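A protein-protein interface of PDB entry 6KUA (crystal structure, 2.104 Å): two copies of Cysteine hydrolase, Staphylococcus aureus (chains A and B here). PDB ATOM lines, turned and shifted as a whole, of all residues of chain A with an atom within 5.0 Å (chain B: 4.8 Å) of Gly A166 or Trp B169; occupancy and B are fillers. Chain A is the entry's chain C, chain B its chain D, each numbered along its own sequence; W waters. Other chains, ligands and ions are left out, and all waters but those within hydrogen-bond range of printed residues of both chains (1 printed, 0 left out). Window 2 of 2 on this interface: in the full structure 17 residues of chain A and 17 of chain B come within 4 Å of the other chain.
Among the printed residues, pairs that only touch across the chains: Trp A169 with Trp B169 (3.3 Å), Asp A135 with His B173 (3.4 Å), Leu A139 with Trp B169 (3.4 Å), Trp A169 with Leu B139 (3.4 Å), Trp A169 with Gly B166 (3.4 Å) and Gly A166 with Trp B169 (3.4 Å).
Gly A166 touches just one residue of chain B: Trp B169 (3.4 Å). Of chain A, only Asp A135, Leu A139, Lys A165, Gly A166 and Trp A169 come within 4 Å of Trp B169. Of the printed residues of chain A, Lys B165 touches Lys A165 (2.4 Å). Of the printed residues of chain B, Lys A165 touches Lys B165 (2.4 Å) and Trp B169 (3.3 Å). Printed residues of chain B within 4 Å of Leu A139: Trp B169 (3.4 Å). Printed residues of chain B within 4 Å of Asp A135: Trp B169 (3.1 Å) and His B173 (3.4 Å). Printed residues of chain A within 4 Å of His B173: Asp A135 (3.4 Å). The nearest printed residue of chain A that does not touch Leu B139 is Leu A139 (4.3 Å).
The backbone NH (N) of Lys A165 sits at hydrogen-bond distance from the side-chain amide oxygen (OD1) of Asn A163, 3.0 Å away. The side-chain amide oxygen (OD1) of Asn A163 is in hydrogen-bond range of the backbone NH (N) of Gly A166, 2.9 Å away.
Leu A139 touches Trp B169, and with the chains exchanged Trp A169 touches Leu B139. Lys B165 touches its own counterpart, Lys A165. Gly A166 touches Trp B169, and with the chains exchanged Trp A169 touches Gly B166. Trp A169 touches its own counterpart, Trp B169. 8 positions are printed for both chains.
Hydrophobic or aromatic side chains of chain B within 4 Å of the printed part of chain A: Leu B139, Trp B169 and His B173. Along chain B the printed residues that touch a printed residue of chain A span positions 139 to 173. Of the 11 printed residues of chain A, 5 touch a printed residue of chain B. Hydrophobic or aromatic side chains of chain A that line the printed part of chain B: Leu A139 and Trp A169. Among the printed residues, 9 pairs touch across the chains.
Water W1 lies within hydrogen-bond range of OD2 of Asp A135 (2.9 Å), ND1 of His B173 (3.1 Å) and NE1 of Trp B169 (3.3 Å).
NE1 of Trp B169 lies within hydrogen-bond range of OD2 of Asp A135 (3.1 Å). The backbone carbonyl oxygen (O) of Lys B165 sits close to the side-chain amino group (NZ) of Lys A165. The backbone NH (N) of Trp B169 lies close to the side-chain amino group (NZ) of Lys A165, at 3.3 Å.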
ATOM      1  N   ASP A 135       9.114 -18.101  18.817  1.00  0.00           N
ATOM      2  CA  ASP A 135       7.711 -17.954  18.458  1.00  0.00           C
ATOM      3  C   ASP A 135       7.508 -17.624  16.984  1.00  0.00           C
ATOM      4  O   ASP A 135       6.407 -17.208  16.602  1.00  0.00           O
ATOM      5  CB  ASP A 135       7.059 -16.876  19.335  1.00  0.00           C
ATOM      6  CG  ASP A 135       7.709 -15.515  19.169  1.00  0.00           C
ATOM      7  OD1 ASP A 135       8.954 -15.450  19.062  1.00  0.00           O
ATOM      8  OD2 ASP A 135       6.977 -14.499  19.134  1.00  0.00           O
ATOM      9  N   LEU A 139       8.675 -22.030  15.984  1.00  0.00           N
ATOM     10  CA  LEU A 139       7.271 -22.396  16.134  1.00  0.00           C
ATOM     11  C   LEU A 139       6.728 -23.055  14.872  1.00  0.00           C
ATOM     12  O   LEU A 139       6.153 -24.144  14.935  1.00  0.00           O
ATOM     13  CB  LEU A 139       6.450 -21.148  16.470  1.00  0.00           C
ATOM     14  CG  LEU A 139       4.934 -21.354  16.398  1.00  0.00           C
ATOM     15  CD1 LEU A 139       4.457 -22.361  17.454  1.00  0.00           C
ATOM     16  CD2 LEU A 139       4.218 -20.013  16.544  1.00  0.00           C
ATOM     17  N   ASN A 163      10.798 -11.230  21.659  1.00  0.00           N
ATOM     18  CA  ASN A 163       9.536 -11.181  22.389  1.00  0.00           C
ATOM     19  C   ASN A 163       9.560 -12.207  23.516  1.00  0.00           C
ATOM     20  O   ASN A 163       9.243 -13.379  23.308  1.00  0.00           O
ATOM     21  CB  ASN A 163       8.388 -11.437  21.418  1.00  0.00           C
ATOM     22  CG  ASN A 163       7.034 -11.252  22.052  1.00  0.00           C
ATOM     23  OD1 ASN A 163       6.909 -11.193  23.281  1.00  0.00           O
ATOM     24  ND2 ASN A 163       5.997 -11.168  21.214  1.00  0.00           N
ATOM     25  N   GLN A 164       9.901 -11.767  24.735  1.00  0.00           N
ATOM     26  CA  GLN A 164       9.926 -12.697  25.860  1.00  0.00           C
ATOM     27  C   GLN A 164       8.548 -13.268  26.160  1.00  0.00           C
ATOM     28  O   GLN A 164       8.434 -14.403  26.643  1.00  0.00           O
ATOM     29  CB  GLN A 164      10.499 -12.024  27.105  1.00  0.00           C
ATOM     30  CG  GLN A 164      11.190 -13.010  28.041  1.00  0.00           C
ATOM     31  CD  GLN A 164      12.370 -13.745  27.382  1.00  0.00           C
ATOM     32  OE1 GLN A 164      12.952 -13.281  26.392  1.00  0.00           O
ATOM     33  NE2 GLN A 164      12.724 -14.894  27.940  1.00  0.00           N
ATOM     34  N   LYS A 165       7.489 -12.507  25.885  1.00  0.00           N
ATOM     35  CA  LYS A 165       6.149 -13.052  26.055  1.00  0.00           C
ATOM     36  C   LYS A 165       5.877 -14.158  25.033  1.00  0.00           C
ATOM     37  O   LYS A 165       5.277 -15.189  25.365  1.00  0.00           O
ATOM     38  CB  LYS A 165       5.126 -11.925  25.945  1.00  0.00           C
ATOM     39  CG  LYS A 165       3.802 -12.206  26.615  1.00  0.00           C
ATOM     40  CD  LYS A 165       2.808 -12.743  25.596  1.00  0.00           C
ATOM     41  CE  LYS A 165       1.389 -12.725  26.132  1.00  0.00           C
ATOM     42  NZ  LYS A 165       0.417 -12.786  25.012  1.00  0.00           N
ATOM     43  N   GLY A 166       6.328 -13.964  23.787  1.00  0.00           N
ATOM     44  CA  GLY A 166       6.145 -14.995  22.773  1.00  0.00           C
ATOM     45  C   GLY A 166       6.995 -16.224  23.035  1.00  0.00           C
ATOM     46  O   GLY A 166       6.554 -17.360  22.815  1.00  0.00           O
ATOM     47  N   HIS A 167       8.221 -16.015  23.517  1.00  0.00           N
ATOM     48  CA  HIS A 167       9.077 -17.131  23.913  1.00  0.00           C
ATOM     49  C   HIS A 167       8.383 -18.013  24.945  1.00  0.00           C
ATOM     50  O   HIS A 167       8.254 -19.232  24.758  1.00  0.00           O
ATOM     51  CB  HIS A 167      10.403 -16.572  24.447  1.00  0.00           C
ATOM     52  CG  HIS A 167      11.337 -17.614  24.974  1.00  0.00           C
ATOM     53  ND1 HIS A 167      12.339 -18.172  24.206  1.00  0.00           N
ATOM     54  CD2 HIS A 167      11.433 -18.190  26.198  1.00  0.00           C
ATOM     55  CE1 HIS A 167      13.013 -19.044  24.938  1.00  0.00           C
ATOM     56  NE2 HIS A 167      12.478 -19.081  26.146  1.00  0.00           N
ATOM     57  N   GLU A 168       7.870 -17.397  26.016  1.00  0.00           N
ATOM     58  CA  GLU A 168       7.174 -18.140  27.067  1.00  0.00           C
ATOM     59  C   GLU A 168       5.899 -18.791  26.540  1.00  0.00           C
ATOM     60  O   GLU A 168       5.622 -19.964  26.829  1.00  0.00           O
ATOM     61  CB  GLU A 168       6.859 -17.204  28.238  1.00  0.00           C
ATOM     62  CG  GLU A 168       7.930 -17.238  29.348  1.00  0.00           C
ATOM     63  CD  GLU A 168       7.968 -15.962  30.191  1.00  0.00           C
ATOM     64  OE1 GLU A 168       8.837 -15.098  29.930  1.00  0.00           O
ATOM     65  OE2 GLU A 168       7.134 -15.825  31.116  1.00  0.00           O
ATOM     66  N   TRP A 169       5.106 -18.047  25.763  1.00  0.00           N
ATOM     67  CA  TRP A 169       3.923 -18.647  25.153  1.00  0.00           C
ATOM     68  C   TRP A 169       4.302 -19.851  24.295  1.00  0.00           C
ATOM     69  O   TRP A 169       3.685 -20.915  24.393  1.00  0.00           O
ATOM     70  CB  TRP A 169       3.147 -17.626  24.302  1.00  0.00           C
ATOM     71  CG  TRP A 169       2.029 -18.340  23.617  1.00  0.00           C
ATOM     72  CD1 TRP A 169       0.799 -18.621  24.132  1.00  0.00           C
ATOM     73  CD2 TRP A 169       2.083 -18.980  22.345  1.00  0.00           C
ATOM     74  NE1 TRP A 169       0.073 -19.374  23.248  1.00  0.00           N
ATOM     75  CE2 TRP A 169       0.847 -19.615  22.144  1.00  0.00           C
ATOM     76  CE3 TRP A 169       3.055 -19.067  21.348  1.00  0.00           C
ATOM     77  CZ2 TRP A 169       0.550 -20.315  20.973  1.00  0.00           C
ATOM     78  CZ3 TRP A 169       2.765 -19.779  20.205  1.00  0.00           C
ATOM     79  CH2 TRP A 169       1.519 -20.386  20.025  1.00  0.00           C
ATOM     80  N   ALA A 170       5.318 -19.695  23.443  1.00  0.00           N
ATOM     81  CA  ALA A 170       5.656 -20.744  22.481  1.00  0.00           C
ATOM     82  C   ALA A 170       6.150 -22.004  23.174  1.00  0.00           C
ATOM     83  O   ALA A 170       5.806 -23.121  22.765  1.00  0.00           O
ATOM     84  CB  ALA A 170       6.703 -20.226  21.494  1.00  0.00           C
ATOM     85  N   LEU A 171       6.956 -21.841  24.231  1.00  0.00           N
ATOM     86  CA  LEU A 171       7.443 -22.988  24.987  1.00  0.00           C
ATOM     87  C   LEU A 171       6.294 -23.792  25.587  1.00  0.00           C
ATOM     88  O   LEU A 171       6.280 -25.029  25.516  1.00  0.00           O
ATOM     89  CB  LEU A 171       8.404 -22.514  26.086  1.00  0.00           C
ATOM     90  CG  LEU A 171       9.839 -22.265  25.608  1.00  0.00           C
ATOM     91  CD1 LEU A 171      10.750 -21.918  26.762  1.00  0.00           C
ATOM     92  CD2 LEU A 171      10.332 -23.503  24.909  1.00  0.00           C
ATOM     93  N   LEU B 139      -4.481 -20.659  14.917  1.00  0.00           N
ATOM     94  CA  LEU B 139      -3.080 -20.342  14.629  1.00  0.00           C
ATOM     95  C   LEU B 139      -2.482 -21.289  13.587  1.00  0.00           C
ATOM     96  O   LEU B 139      -1.805 -20.845  12.654  1.00  0.00           O
ATOM     97  CB  LEU B 139      -2.255 -20.385  15.915  1.00  0.00           C
ATOM     98  CG  LEU B 139      -0.742 -20.411  15.704  1.00  0.00           C
ATOM     99  CD1 LEU B 139      -0.266 -19.070  15.199  1.00  0.00           C
ATOM    100  CD2 LEU B 139      -0.031 -20.800  17.015  1.00  0.00           C
ATOM    101  N   LYS B 165      -3.470 -14.757  27.338  1.00  0.00           N
ATOM    102  CA  LYS B 165      -2.113 -14.464  26.888  1.00  0.00           C
ATOM    103  C   LYS B 165      -1.890 -14.975  25.468  1.00  0.00           C
ATOM    104  O   LYS B 165      -1.374 -14.253  24.608  1.00  0.00           O
ATOM    105  CB  LYS B 165      -1.097 -15.084  27.850  1.00  0.00           C
ATOM    106  CG  LYS B 165      -0.880 -14.290  29.133  1.00  0.00           C
ATOM    107  CD  LYS B 165       0.478 -14.589  29.752  1.00  0.00           C
ATOM    108  CE  LYS B 165       0.615 -16.061  30.152  1.00  0.00           C
ATOM    109  NZ  LYS B 165       1.979 -16.399  30.691  1.00  0.00           N
ATOM    110  N   GLY B 166      -2.283 -16.223  25.209  1.00  0.00           N
ATOM    111  CA  GLY B 166      -2.114 -16.783  23.880  1.00  0.00           C
ATOM    112  C   GLY B 166      -2.971 -16.084  22.846  1.00  0.00           C
ATOM    113  O   GLY B 166      -2.530 -15.843  21.718  1.00  0.00           O
ATOM    114  N   HIS B 167      -4.209 -15.748  23.219  1.00  0.00           N
ATOM    115  CA  HIS B 167      -5.077 -14.982  22.333  1.00  0.00           C
ATOM    116  C   HIS B 167      -4.381 -13.710  21.874  1.00  0.00           C
ATOM    117  O   HIS B 167      -4.301 -13.422  20.671  1.00  0.00           O
ATOM    118  CB  HIS B 167      -6.384 -14.667  23.060  1.00  0.00           C
ATOM    119  CG  HIS B 167      -7.348 -13.849  22.257  1.00  0.00           C
ATOM    120  ND1 HIS B 167      -8.213 -14.410  21.341  1.00  0.00           N
ATOM    121  CD2 HIS B 167      -7.591 -12.515  22.242  1.00  0.00           C
ATOM    122  CE1 HIS B 167      -8.952 -13.454  20.799  1.00  0.00           C
ATOM    123  NE2 HIS B 167      -8.596 -12.298  21.331  1.00  0.00           N
ATOM    124  N   GLU B 168      -3.821 -12.962  22.830  1.00  0.00           N
ATOM    125  CA  GLU B 168      -3.197 -11.683  22.507  1.00  0.00           C
ATOM    126  C   GLU B 168      -1.902 -11.885  21.742  1.00  0.00           C
ATOM    127  O   GLU B 168      -1.584 -11.101  20.839  1.00  0.00           O
ATOM    128  CB  GLU B 168      -2.939 -10.880  23.788  1.00  0.00           C
ATOM    129  CG  GLU B 168      -4.209 -10.281  24.407  1.00  0.00           C
ATOM    130  CD  GLU B 168      -4.041  -9.861  25.873  1.00  0.00           C
ATOM    131  OE1 GLU B 168      -2.900  -9.898  26.396  1.00  0.00           O
ATOM    132  OE2 GLU B 168      -5.066  -9.489  26.501  1.00  0.00           O
ATOM    133  N   TRP B 169      -1.123 -12.907  22.112  1.00  0.00           N
ATOM    134  CA  TRP B 169       0.071 -13.230  21.341  1.00  0.00           C
ATOM    135  C   TRP B 169      -0.307 -13.602  19.913  1.00  0.00           C
ATOM    136  O   TRP B 169       0.304 -13.121  18.952  1.00  0.00           O
ATOM    137  CB  TRP B 169       0.875 -14.373  21.992  1.00  0.00           C
ATOM    138  CG  TRP B 169       2.021 -14.775  21.076  1.00  0.00           C
ATOM    139  CD1 TRP B 169       3.264 -14.227  21.038  1.00  0.00           C
ATOM    140  CD2 TRP B 169       1.971 -15.731  20.003  1.00  0.00           C
ATOM    141  NE1 TRP B 169       4.001 -14.795  20.021  1.00  0.00           N
ATOM    142  CE2 TRP B 169       3.224 -15.718  19.372  1.00  0.00           C
ATOM    143  CE3 TRP B 169       0.988 -16.605  19.527  1.00  0.00           C
ATOM    144  CZ2 TRP B 169       3.521 -16.542  18.292  1.00  0.00           C
ATOM    145  CZ3 TRP B 169       1.283 -17.413  18.435  1.00  0.00           C
ATOM    146  CH2 TRP B 169       2.533 -17.376  17.838  1.00  0.00           C
ATOM    147  N   ALA B 170      -1.325 -14.454  19.755  1.00  0.00           N
ATOM    148  CA  ALA B 170      -1.655 -14.949  18.416  1.00  0.00           C
ATOM    149  C   ALA B 170      -2.153 -13.829  17.496  1.00  0.00           C
ATOM    150  O   ALA B 170      -1.801 -13.788  16.310  1.00  0.00           O
ATOM    151  CB  ALA B 170      -2.685 -16.078  18.510  1.00  0.00           C
ATOM    152  N   LEU B 171      -2.969 -12.903  18.012  1.00  0.00           N
ATOM    153  CA  LEU B 171      -3.440 -11.832  17.132  1.00  0.00           C
ATOM    154  C   LEU B 171      -2.286 -10.957  16.654  1.00  0.00           C
ATOM    155  O   LEU B 171      -2.302 -10.478  15.510  1.00  0.00           O
ATOM    156  CB  LEU B 171      -4.507 -10.988  17.824  1.00  0.00           C
ATOM    157  CG  LEU B 171      -5.820 -11.720  18.122  1.00  0.00           C
ATOM    158  CD1 LEU B 171      -6.577 -10.956  19.180  1.00  0.00           C
ATOM    159  CD2 LEU B 171      -6.682 -11.877  16.870  1.00  0.00           C
ATOM    160  N   ALA B 172      -1.272 -10.750  17.500  1.00  0.00           N
ATOM    161  CA  ALA B 172      -0.113  -9.961  17.080  1.00  0.00           C
ATOM    162  C   ALA B 172       0.728 -10.723  16.062  1.00  0.00           C
ATOM    163  O   ALA B 172       1.227 -10.136  15.086  1.00  0.00           O
ATOM    164  CB  ALA B 172       0.728  -9.572  18.300  1.00  0.00           C
ATOM    165  N   HIS B 173       0.875 -12.037  16.265  1.00  0.00           N
ATOM    166  CA  HIS B 173       1.565 -12.894  15.298  1.00  0.00           C
ATOM    167  C   HIS B 173       0.930 -12.798  13.908  1.00  0.00           C
ATOM    168  O   HIS B 173       1.632 -12.610  12.903  1.00  0.00           O
ATOM    169  CB  HIS B 173       1.540 -14.338  15.800  1.00  0.00           C
ATOM    170  CG  HIS B 173       2.362 -15.285  14.972  1.00  0.00           C
ATOM    171  ND1 HIS B 173       3.737 -15.353  15.061  1.00  0.00           N
ATOM    172  CD2 HIS B 173       1.998 -16.217  14.056  1.00  0.00           C
ATOM    173  CE1 HIS B 173       4.184 -16.279  14.231  1.00  0.00           C
ATOM    174  NE2 HIS B 173       3.152 -16.818  13.609  1.00  0.00           N
HETATM  175  O   HOH W   1       5.061 -13.558  17.166  1.00  0.00           O
